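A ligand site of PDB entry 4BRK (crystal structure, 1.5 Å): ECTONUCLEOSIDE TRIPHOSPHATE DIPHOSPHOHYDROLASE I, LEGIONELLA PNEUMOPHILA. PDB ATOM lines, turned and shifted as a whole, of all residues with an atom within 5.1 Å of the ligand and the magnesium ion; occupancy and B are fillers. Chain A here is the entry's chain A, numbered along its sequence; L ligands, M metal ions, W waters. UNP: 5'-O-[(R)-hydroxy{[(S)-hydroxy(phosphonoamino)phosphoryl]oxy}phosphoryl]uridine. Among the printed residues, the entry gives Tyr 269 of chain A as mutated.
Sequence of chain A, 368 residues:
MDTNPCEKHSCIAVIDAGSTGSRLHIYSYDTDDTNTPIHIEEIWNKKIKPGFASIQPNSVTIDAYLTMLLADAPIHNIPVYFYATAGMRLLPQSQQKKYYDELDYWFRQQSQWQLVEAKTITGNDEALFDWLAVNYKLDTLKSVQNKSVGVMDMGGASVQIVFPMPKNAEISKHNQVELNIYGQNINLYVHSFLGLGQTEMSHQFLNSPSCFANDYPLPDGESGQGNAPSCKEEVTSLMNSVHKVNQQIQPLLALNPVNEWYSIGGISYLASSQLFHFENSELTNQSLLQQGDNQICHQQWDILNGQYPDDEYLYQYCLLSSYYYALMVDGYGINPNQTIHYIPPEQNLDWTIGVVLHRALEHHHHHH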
ATOM      1  N   ASP A  16      12.512  10.696 -14.738  1.00  0.00           N
ATOM      2  CA  ASP A  16      13.173   9.822 -15.705  1.00  0.00           C
ATOM      3  C   ASP A  16      14.572   9.514 -15.148  1.00  0.00           C
ATOM      4  O   ASP A  16      15.469  10.356 -15.235  1.00  0.00           O
ATOM      5  CB  ASP A  16      13.265  10.567 -17.054  1.00  0.00           C
ATOM      6  CG  ASP A  16      14.184   9.885 -18.104  1.00  0.00           C
ATOM      7  OD1 ASP A  16      14.635   8.754 -17.846  1.00  0.00           O
ATOM      8  OD2 ASP A  16      14.419  10.536 -19.136  1.00  0.00           O
ATOM      9  N   ALA A  17      14.727   8.339 -14.529  1.00  0.00           N
ATOM     10  CA  ALA A  17      16.053   7.901 -13.986  1.00  0.00           C
ATOM     11  C   ALA A  17      16.697   7.093 -15.139  1.00  0.00           C
ATOM     12  O   ALA A  17      16.662   5.831 -15.187  1.00  0.00           O
ATOM     13  CB  ALA A  17      15.898   7.068 -12.684  1.00  0.00           C
ATOM     14  N   GLY A  18      17.311   7.836 -16.045  1.00  0.00           N
ATOM     15  CA  GLY A  18      17.869   7.246 -17.271  1.00  0.00           C
ATOM     16  C   GLY A  18      19.332   6.842 -17.091  1.00  0.00           C
ATOM     17  O   GLY A  18      19.963   7.122 -16.000  1.00  0.00           O
ATOM     18  N   SER A  19      19.877   6.164 -18.114  1.00  0.00           N
ATOM     19  CA  SER A  19      21.191   5.586 -17.928  1.00  0.00           C
ATOM     20  C   SER A  19      22.294   6.667 -17.697  1.00  0.00           C
ATOM     21  O   SER A  19      23.267   6.383 -17.040  1.00  0.00           O
ATOM     22  CB  SER A  19      21.550   4.680 -19.115  1.00  0.00           C
ATOM     23  OG  SER A  19      21.806   5.456 -20.290  1.00  0.00           O
ATOM     24  N   THR A  20      22.134   7.871 -18.262  1.00  0.00           N
ATOM     25  CA  THR A  20      23.217   8.906 -18.171  1.00  0.00           C
ATOM     26  C   THR A  20      22.892  10.005 -17.164  1.00  0.00           C
ATOM     27  O   THR A  20      23.728  10.867 -16.892  1.00  0.00           O
ATOM     28  CB  THR A  20      23.552   9.542 -19.530  1.00  0.00           C
ATOM     29  OG1 THR A  20      22.439  10.318 -19.990  1.00  0.00           O
ATOM     30  CG2 THR A  20      23.909   8.466 -20.592  1.00  0.00           C
ATOM     31  N   GLY A  21      21.684   9.962 -16.593  1.00  0.00           N
ATOM     32  CA  GLY A  21      21.318  11.030 -15.649  1.00  0.00           C
ATOM     33  C   GLY A  21      19.854  10.898 -15.247  1.00  0.00           C
ATOM     34  O   GLY A  21      19.120  10.099 -15.840  1.00  0.00           O
ATOM     35  N   ARG A  23      16.121  13.054 -14.515  1.00  0.00           N
ATOM     36  CA  ARG A  23      15.413  14.315 -14.792  1.00  0.00           C
ATOM     37  C   ARG A  23      14.131  14.313 -14.027  1.00  0.00           C
ATOM     38  O   ARG A  23      13.243  13.494 -14.256  1.00  0.00           O
ATOM     39  CB  ARG A  23      15.133  14.517 -16.269  1.00  0.00           C
ATOM     40  CG  ARG A  23      16.411  14.359 -17.152  1.00  0.00           C
ATOM     41  CD  ARG A  23      16.529  12.910 -17.624  1.00  0.00           C
ATOM     42  NE  ARG A  23      17.929  12.619 -18.086  1.00  0.00           N
ATOM     43  CZ  ARG A  23      18.301  11.554 -18.784  1.00  0.00           C
ATOM     44  NH1 ARG A  23      17.379  10.605 -19.102  1.00  0.00           N
ATOM     45  NH2 ARG A  23      19.605  11.399 -19.085  1.00  0.00           N
ATOM     46  N   THR A  85      15.170   3.390 -16.223  1.00  0.00           N
ATOM     47  CA  THR A  85      15.161   2.750 -17.516  1.00  0.00           C
ATOM     48  C   THR A  85      16.401   1.834 -17.700  1.00  0.00           C
ATOM     49  O   THR A  85      16.728   1.073 -16.744  1.00  0.00           O
ATOM     50  CB  THR A  85      14.932   3.774 -18.631  1.00  0.00           C
ATOM     51  OG1 THR A  85      15.944   4.813 -18.530  1.00  0.00           O
ATOM     52  CG2 THR A  85      13.571   4.404 -18.482  1.00  0.00           C
ATOM     53  N   ALA A  86      17.034   1.827 -18.898  1.00  0.00           N
ATOM     54  CA  ALA A  86      17.956   0.770 -19.248  1.00  0.00           C
ATOM     55  C   ALA A  86      19.219   0.740 -18.384  1.00  0.00           C
ATOM     56  O   ALA A  86      19.817  -0.325 -18.276  1.00  0.00           O
ATOM     57  CB  ALA A  86      18.371   0.863 -20.715  1.00  0.00           C
ATOM     58  N   GLY A  87      19.648   1.872 -17.784  1.00  0.00           N
ATOM     59  CA  GLY A  87      20.830   1.798 -16.887  1.00  0.00           C
ATOM     60  C   GLY A  87      20.576   0.823 -15.739  1.00  0.00           C
ATOM     61  O   GLY A  87      21.429  -0.012 -15.393  1.00  0.00           O
ATOM     62  N   GLU A 126       8.428   1.703 -21.391  1.00  0.00           N
ATOM     63  CA  GLU A 126       9.197   2.876 -21.797  1.00  0.00           C
ATOM     64  C   GLU A 126       8.794   3.297 -23.247  1.00  0.00           C
ATOM     65  O   GLU A 126       8.561   4.479 -23.546  1.00  0.00           O
ATOM     66  CB  GLU A 126      10.696   2.578 -21.634  1.00  0.00           C
ATOM     67  CG  GLU A 126      11.606   3.772 -21.944  1.00  0.00           C
ATOM     68  CD  GLU A 126      13.046   3.393 -21.733  1.00  0.00           C
ATOM     69  OE1 GLU A 126      13.330   2.155 -21.555  1.00  0.00           O
ATOM     70  OE2 GLU A 126      13.977   4.234 -21.882  1.00  0.00           O
ATOM     71  N   ASP A 153      13.115   6.273 -29.636  1.00  0.00           N
ATOM     72  CA  ASP A 153      13.802   6.991 -28.572  1.00  0.00           C
ATOM     73  C   ASP A 153      15.245   6.436 -28.516  1.00  0.00           C
ATOM     74  O   ASP A 153      15.491   5.233 -28.251  1.00  0.00           O
ATOM     75  CB  ASP A 153      13.087   6.697 -27.213  1.00  0.00           C
ATOM     76  CG  ASP A 153      13.723   7.390 -25.980  1.00  0.00           C
ATOM     77  OD1 ASP A 153      14.860   7.928 -26.082  1.00  0.00           O
ATOM     78  OD2 ASP A 153      13.079   7.312 -24.869  1.00  0.00           O
ATOM     79  N   MET A 154      16.189   7.330 -28.855  1.00  0.00           N
ATOM     80  CA  MET A 154      17.584   7.000 -29.002  1.00  0.00           C
ATOM     81  C   MET A 154      18.345   7.281 -27.715  1.00  0.00           C
ATOM     82  O   MET A 154      18.993   8.338 -27.597  1.00  0.00           O
ATOM     83  CB  MET A 154      18.091   7.868 -30.186  1.00  0.00           C
ATOM     84  CG  MET A 154      17.389   7.602 -31.547  1.00  0.00           C
ATOM     85  SD  MET A 154      17.540   5.878 -31.978  1.00  0.00           S
ATOM     86  CE  MET A 154      17.068   5.985 -33.742  1.00  0.00           C
ATOM     87  N   GLY A 155      18.236   6.366 -26.750  1.00  0.00           N
ATOM     88  CA  GLY A 155      18.808   6.637 -25.379  1.00  0.00           C
ATOM     89  C   GLY A 155      20.258   6.136 -25.301  1.00  0.00           C
ATOM     90  O   GLY A 155      20.897   5.722 -26.309  1.00  0.00           O
ATOM     91  N   GLY A 156      20.794   6.160 -24.082  1.00  0.00           N
ATOM     92  CA  GLY A 156      22.164   5.840 -23.788  1.00  0.00           C
ATOM     93  C   GLY A 156      22.416   4.373 -23.615  1.00  0.00           C
ATOM     94  O   GLY A 156      23.561   3.926 -23.921  1.00  0.00           O
ATOM     95  N   ALA A 157      21.449   3.611 -23.063  1.00  0.00           N
ATOM     96  CA  ALA A 157      21.686   2.171 -22.809  1.00  0.00           C
ATOM     97  C   ALA A 157      20.712   1.298 -23.593  1.00  0.00           C
ATOM     98  O   ALA A 157      21.077   0.181 -23.954  1.00  0.00           O
ATOM     99  CB  ALA A 157      21.661   1.826 -21.310  1.00  0.00           C
ATOM    100  N   SER A 158      19.500   1.781 -23.897  1.00  0.00           N
ATOM    101  CA  SER A 158      18.644   1.051 -24.839  1.00  0.00           C
ATOM    102  C   SER A 158      18.068   2.066 -25.856  1.00  0.00           C
ATOM    103  O   SER A 158      18.173   3.312 -25.697  1.00  0.00           O
ATOM    104  CB  SER A 158      17.457   0.327 -24.113  1.00  0.00           C
ATOM    105  OG  SER A 158      16.523   1.295 -23.560  1.00  0.00           O
ATOM    106  N   GLN A 198      23.409   4.525 -27.074  1.00  0.00           N
ATOM    107  CA  GLN A 198      24.668   5.059 -27.585  1.00  0.00           C
ATOM    108  C   GLN A 198      25.893   4.752 -26.678  1.00  0.00           C
ATOM    109  O   GLN A 198      26.977   4.509 -27.209  1.00  0.00           O
ATOM    110  CB  GLN A 198      24.586   6.555 -27.957  1.00  0.00           C
ATOM    111  CG  GLN A 198      24.229   7.478 -26.882  1.00  0.00           C
ATOM    112  CD  GLN A 198      24.554   8.906 -27.333  1.00  0.00           C
ATOM    113  OE1 GLN A 198      23.715   9.624 -27.977  1.00  0.00           O
ATOM    114  NE2 GLN A 198      25.782   9.323 -27.010  1.00  0.00           N
ATOM    115  N   THR A 199      25.741   4.782 -25.342  1.00  0.00           N
ATOM    116  CA  THR A 199      26.909   4.617 -24.502  1.00  0.00           C
ATOM    117  C   THR A 199      27.364   3.179 -24.588  1.00  0.00           C
ATOM    118  O   THR A 199      28.574   2.891 -24.752  1.00  0.00           O
ATOM    119  CB  THR A 199      26.616   4.993 -23.009  1.00  0.00           C
ATOM    120  OG1 THR A 199      26.050   6.299 -22.998  1.00  0.00           O
ATOM    121  CG2 THR A 199      27.895   4.895 -22.220  1.00  0.00           C
ATOM    122  N   GLY A 265      15.209  11.331 -27.335  1.00  0.00           N
ATOM    123  CA  GLY A 265      16.472  10.935 -26.724  1.00  0.00           C
ATOM    124  C   GLY A 265      17.637  11.733 -27.255  1.00  0.00           C
ATOM    125  O   GLY A 265      17.522  12.858 -27.861  1.00  0.00           O
ATOM    126  N   GLY A 266      18.820  11.162 -27.059  1.00  0.00           N
ATOM    127  CA  GLY A 266      20.077  11.909 -27.230  1.00  0.00           C
ATOM    128  C   GLY A 266      20.338  12.338 -28.646  1.00  0.00           C
ATOM    129  O   GLY A 266      21.160  13.270 -28.886  1.00  0.00           O
ATOM    130  N   TYR A 269      20.266  16.097 -29.411  1.00  0.00           N
ATOM    131  CA  TYR A 269      21.443  16.950 -29.150  1.00  0.00           C
ATOM    132  C   TYR A 269      22.381  16.940 -30.349  1.00  0.00           C
ATOM    133  O   TYR A 269      22.879  17.982 -30.778  1.00  0.00           O
ATOM    134  CB  TYR A 269      22.215  16.453 -27.946  1.00  0.00           C
ATOM    135  CG  TYR A 269      21.494  16.433 -26.641  1.00  0.00           C
ATOM    136  CD1 TYR A 269      20.980  17.583 -26.017  1.00  0.00           C
ATOM    137  CD2 TYR A 269      21.269  15.171 -26.003  1.00  0.00           C
ATOM    138  CE1 TYR A 269      20.315  17.496 -24.762  1.00  0.00           C
ATOM    139  CE2 TYR A 269      20.631  15.078 -24.768  1.00  0.00           C
ATOM    140  CZ  TYR A 269      20.132  16.242 -24.167  1.00  0.00           C
ATOM    141  OH  TYR A 269      19.512  16.111 -22.905  1.00  0.00           O
ATOM    142  N   TYR A 313      30.961  16.994 -26.522  1.00  0.00           N
ATOM    143  CA  TYR A 313      30.344  15.792 -27.155  1.00  0.00           C
ATOM    144  C   TYR A 313      30.812  15.619 -28.588  1.00  0.00           C
ATOM    145  O   TYR A 313      30.693  14.537 -29.192  1.00  0.00           O
ATOM    146  CB  TYR A 313      28.804  15.914 -27.162  1.00  0.00           C
ATOM    147  CG  TYR A 313      28.294  15.951 -25.739  1.00  0.00           C
ATOM    148  CD1 TYR A 313      28.305  14.803 -24.977  1.00  0.00           C
ATOM    149  CD2 TYR A 313      27.808  17.129 -25.186  1.00  0.00           C
ATOM    150  CE1 TYR A 313      27.891  14.850 -23.676  1.00  0.00           C
ATOM    151  CE2 TYR A 313      27.372  17.183 -23.878  1.00  0.00           C
ATOM    152  CZ  TYR A 313      27.411  16.035 -23.128  1.00  0.00           C
ATOM    153  OH  TYR A 313      26.965  16.017 -21.828  1.00  0.00           O
ATOM    154  N   GLN A 316      32.602  12.548 -30.482  1.00  0.00           N
ATOM    155  CA  GLN A 316      31.900  11.299 -30.755  1.00  0.00           C
ATOM    156  C   GLN A 316      30.955  11.401 -31.938  1.00  0.00           C
ATOM    157  O   GLN A 316      30.261  10.429 -32.267  1.00  0.00           O
ATOM    158  CB  GLN A 316      31.146  10.838 -29.521  1.00  0.00           C
ATOM    159  CG  GLN A 316      31.356   9.358 -29.350  1.00  0.00           C
ATOM    160  CD  GLN A 316      30.710   8.794 -28.102  1.00  0.00           C
ATOM    161  OE1 GLN A 316      29.581   9.121 -27.782  1.00  0.00           O
ATOM    162  NE2 GLN A 316      31.422   7.924 -27.419  1.00  0.00           N
ATOM    163  N   LEU A 320      28.628   8.663 -33.788  1.00  0.00           N
ATOM    164  CA  LEU A 320      27.179   8.691 -33.590  1.00  0.00           C
ATOM    165  C   LEU A 320      26.405   8.817 -34.917  1.00  0.00           C
ATOM    166  O   LEU A 320      25.334   8.154 -35.109  1.00  0.00           O
ATOM    167  CB  LEU A 320      26.728   9.773 -32.618  1.00  0.00           C
ATOM    168  CG  LEU A 320      27.240   9.577 -31.186  1.00  0.00           C
ATOM    169  CD1 LEU A 320      26.615  10.691 -30.372  1.00  0.00           C
ATOM    170  CD2 LEU A 320      26.851   8.197 -30.620  1.00  0.00           C
ATOM    171  N   TRP A 351       9.920  10.600 -22.246  1.00  0.00           N
ATOM    172  CA  TRP A 351       8.693   9.799 -22.135  1.00  0.00           C
ATOM    173  C   TRP A 351       7.803  10.106 -20.944  1.00  0.00           C
ATOM    174  O   TRP A 351       6.710   9.482 -20.792  1.00  0.00           O
ATOM    175  CB  TRP A 351       9.053   8.274 -22.181  1.00  0.00           C
ATOM    176  CG  TRP A 351      10.197   7.941 -21.216  1.00  0.00           C
ATOM    177  CD1 TRP A 351      11.555   7.878 -21.536  1.00  0.00           C
ATOM    178  CD2 TRP A 351      10.111   7.796 -19.789  1.00  0.00           C
ATOM    179  NE1 TRP A 351      12.302   7.599 -20.381  1.00  0.00           N
ATOM    180  CE2 TRP A 351      11.460   7.562 -19.285  1.00  0.00           C
ATOM    181  CE3 TRP A 351       9.025   7.819 -18.846  1.00  0.00           C
ATOM    182  CZ2 TRP A 351      11.721   7.332 -17.924  1.00  0.00           C
ATOM    183  CZ3 TRP A 351       9.310   7.558 -17.462  1.00  0.00           C
ATOM    184  CH2 TRP A 351      10.628   7.359 -17.021  1.00  0.00           C
HETATM  185  O2G UNP L   1      18.841   4.292 -22.201  1.00  0.00           O
HETATM  186  PG  UNP L   1      18.343   5.429 -21.381  1.00  0.00           P
HETATM  187  O3G UNP L   1      17.107   6.052 -21.975  1.00  0.00           O
HETATM  188  O1G UNP L   1      18.193   5.067 -19.917  1.00  0.00           O
HETATM  189  N2B UNP L   1      19.540   6.600 -21.442  1.00  0.00           N
HETATM  190  PB  UNP L   1      19.332   8.294 -21.287  1.00  0.00           P
HETATM  191  O1B UNP L   1      20.202   8.846 -20.214  1.00  0.00           O
HETATM  192  O3B UNP L   1      17.879   8.620 -21.148  1.00  0.00           O
HETATM  193  O3A UNP L   1      19.880   8.816 -22.713  1.00  0.00           O
HETATM  194  PA  UNP L   1      19.555  10.207 -23.439  1.00  0.00           P
HETATM  195  O1A UNP L   1      19.353  11.252 -22.394  1.00  0.00           O
HETATM  196  O2A UNP L   1      18.479   9.935 -24.431  1.00  0.00           O
HETATM  197  O5' UNP L   1      20.948  10.487 -24.187  1.00  0.00           O
HETATM  198  C5' UNP L   1      22.153  10.598 -23.452  1.00  0.00           C
HETATM  199  C4' UNP L   1      23.201  11.143 -24.404  1.00  0.00           C
HETATM  200  C3' UNP L   1      24.558  11.223 -23.710  1.00  0.00           C
HETATM  201  O3' UNP L   1      25.239   9.932 -23.659  1.00  0.00           O
HETATM  202  C2' UNP L   1      25.283  12.297 -24.490  1.00  0.00           C
HETATM  203  O2' UNP L   1      25.907  11.685 -25.637  1.00  0.00           O
HETATM  204  O4' UNP L   1      22.919  12.509 -24.863  1.00  0.00           O
HETATM  205  C1' UNP L   1      24.199  13.195 -25.052  1.00  0.00           C
HETATM  206  N1  UNP L   1      24.048  14.481 -24.360  1.00  0.00           N
HETATM  207  C2  UNP L   1      24.359  15.641 -25.085  1.00  0.00           C
HETATM  208  O2  UNP L   1      24.788  15.580 -26.252  1.00  0.00           O
HETATM  209  C6  UNP L   1      23.544  14.553 -23.100  1.00  0.00           C
HETATM  210  C5  UNP L   1      23.310  15.806 -22.518  1.00  0.00           C
HETATM  211  C4  UNP L   1      23.640  16.950 -23.282  1.00  0.00           C
HETATM  212  N3  UNP L   1      24.170  16.837 -24.512  1.00  0.00           N
HETATM  213  O4  UNP L   1      23.495  18.119 -22.839  1.00  0.00           O
HETATM  214 MG    MG M   1      16.099   7.802 -21.813  1.00  0.00          MG
HETATM  215  O   HOH W   1      25.576  16.628 -28.867  1.00  0.00           O
HETATM  216  O   HOH W   2      25.942  13.775 -28.515  1.00  0.00           O
HETATM  217  O   HOH W   3      21.115  18.606 -20.444  1.00  0.00           O
HETATM  218  O   HOH W   4      23.333  12.781 -20.492  1.00  0.00           O
HETATM  219  O   HOH W   5      15.392   7.273 -19.895  1.00  0.00           O
HETATM  220  O   HOH W   6      28.377  11.347 -26.738  1.00  0.00           O
HETATM  221  O   HOH W   7      16.387   8.420 -23.816  1.00  0.00           O
HETATM  222  O   HOH W   8      27.117  10.156 -21.698  1.00  0.00           O
HETATM  223  O   HOH W   9      25.014  18.832 -26.733  1.00  0.00           O
HETATM  224  O   HOH W  10      16.139   4.869 -24.346  1.00  0.00           O
HETATM  225  O   HOH W  11      14.367   6.892 -22.573  1.00  0.00           O
HETATM  226  O   HOH W  12      16.675  11.940 -22.046  1.00  0.00           O
HETATM  227  O   HOH W  13      19.893  13.831 -21.597  1.00  0.00           O
HETATM  228  O   HOH W  14      21.395   8.953 -26.592  1.00  0.00           O
HETATM  229  O   HOH W  15      16.282   3.044 -21.617  1.00  0.00           O
HETATM  230  O   HOH W  16      15.080   9.675 -21.481  1.00  0.00           O
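The side-chain hydroxyl of Thr 85 sits at hydrogen-bond distance from an oxygen (O1G) of the ligand, 2.7 Å away.
An oxygen (O1B) of the ligand is in hydrogen-bond range of the backbone NH (N) of Thr 20, at 2.9 Å.
An oxygen (O1B) of the ligand lies within hydrogen-bond range of the side-chain hydroxyl of Thr 20, at 2.7 Å.
An oxygen (O1G) of the ligand is in hydrogen-bond range of the backbone NH (N) of Ser 19, at 2.7 Å.
The side-chain hydroxyl (OG) of Ser 19 is in hydrogen-bond range of a nitrogen (N2B) of the ligand (2.8 Å).
The side-chain amide nitrogen (NE2) of Gln 198 lies within hydrogen-bond range of an oxygen (O2') of the ligand, 2.7 Å away.
N of Ala 157 is in hydrogen-bond range of O2G of the ligand, at 2.8 Å.
An oxygen (O1B) of the ligand lies within salt-bridge range of the guanidinium group (NH2) of Arg 23 (2.9 Å).
N of Gly 266 lies within hydrogen-bond range of O2A of the ligand (2.9 Å).
N of Gly 156 lies within hydrogen-bond range of O3A of the ligand (3.1 Å).
An oxygen (O2G) of the ligand is in hydrogen-bond range of the backbone NH of Ser 158 (3.1 Å).
The backbone NH (N) of Thr 85 lies within hydrogen-bond range of the backbone carbonyl oxygen (O) of Ala 17 (3.0 Å).
The guanidinium group (NH2) of Arg 23 sits at hydrogen-bond distance from the side-chain hydroxyl (OG1) of Thr 20 (3.2 Å).
N of Gln 198 sits at hydrogen-bond distance from O of Gly 156 (3.2 Å).
O of Gly 155 lies within hydrogen-bond range of N of Gln 198.
The guanidinium group (NH1) of Arg 23 lies within salt-bridge range of the side-chain carboxylate (OD2) of Asp 16, at 3.0 Å.
The backbone NH (N) of Gly 266 sits at hydrogen-bond distance from the backbone carbonyl oxygen (O) of Met 154 (2.9 Å).
The backbone NH (N) of Thr 199 sits at hydrogen-bond distance from the backbone carbonyl oxygen (O) of Gly 156, 2.7 Å away.
N of Gly 18 sits close to OD1 of Asp 16 (3.4 Å).
Gly 18 touches the ligand (CA to O1G, 3.4 Å).
N of Ala 86 touches O1G of the ligand, 3.6 Å away.
Glu 126 touches the ligand (OE2 to O3G, 3.6 Å).
Met 154 touches the ligand.
CA of Gly 155 touches O2A of the ligand, at 3.4 Å.
OG1 of Thr 199 touches O3' of the ligand, at 3.8 Å.
Gly 265 touches the ligand (CA to O2A, 3.2 Å).
Tyr 269 touches the ligand.
Tyr 313 touches the ligand.
Hydrophobic or aromatic side chains within 4 Å of the ligand: Ala 86, Ala 157, Tyr 269 and Tyr 313.
Of the 26 residues printed, 18 come within 4 Å of the ligand.
No residue comes within 4 Å of the magnesium ion.
The nearest printed residue that does not touch the magnesium ion is Trp 351 (4.1 Å).
The magnesium ion is bound by an oxygen (O3G) of the ligand (2.0 Å), an oxygen (O3B) of the ligand (2.1 Å), water W11 (2.1 Å), water W5 (2.1 Å), water W7 (2.1 Å) and water W16 (2.2 Å).
Water W11 lies within hydrogen-bond range of OD2 of Asp 153, OE2 of Glu 126 and NE1 of Trp 351.
Water W5 lies within hydrogen-bond range of the side-chain carboxylate (OD1) of Asp 16 (2.6 Å), the side-chain hydroxyl (OG1) of Thr 85 (2.9 Å) and the indole nitrogen (NE1) of Trp 351 (3.1 Å).
Water W7 bridges an oxygen (O2A) of the ligand and the side-chain carboxylate (OD1) of Asp 153.
Water W6 lies within hydrogen-bond range of an oxygen (O2') of the ligand, the side-chain amide oxygen of Gln 316 and the side-chain amide nitrogen of Gln 198.
Water W13 lies within hydrogen-bond range of the side-chain hydroxyl (OH) of Tyr 269 (2.7 Å) and an oxygen (O1A) of the ligand (2.8 Å).
Water W15 lies within hydrogen-bond range of the side-chain carboxylate of Glu 126 (2.6 Å), the side-chain hydroxyl of Ser 158 (2.6 Å), an oxygen (O2G) of the ligand (2.9 Å) and the backbone NH of Ala 86 (3.1 Å).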
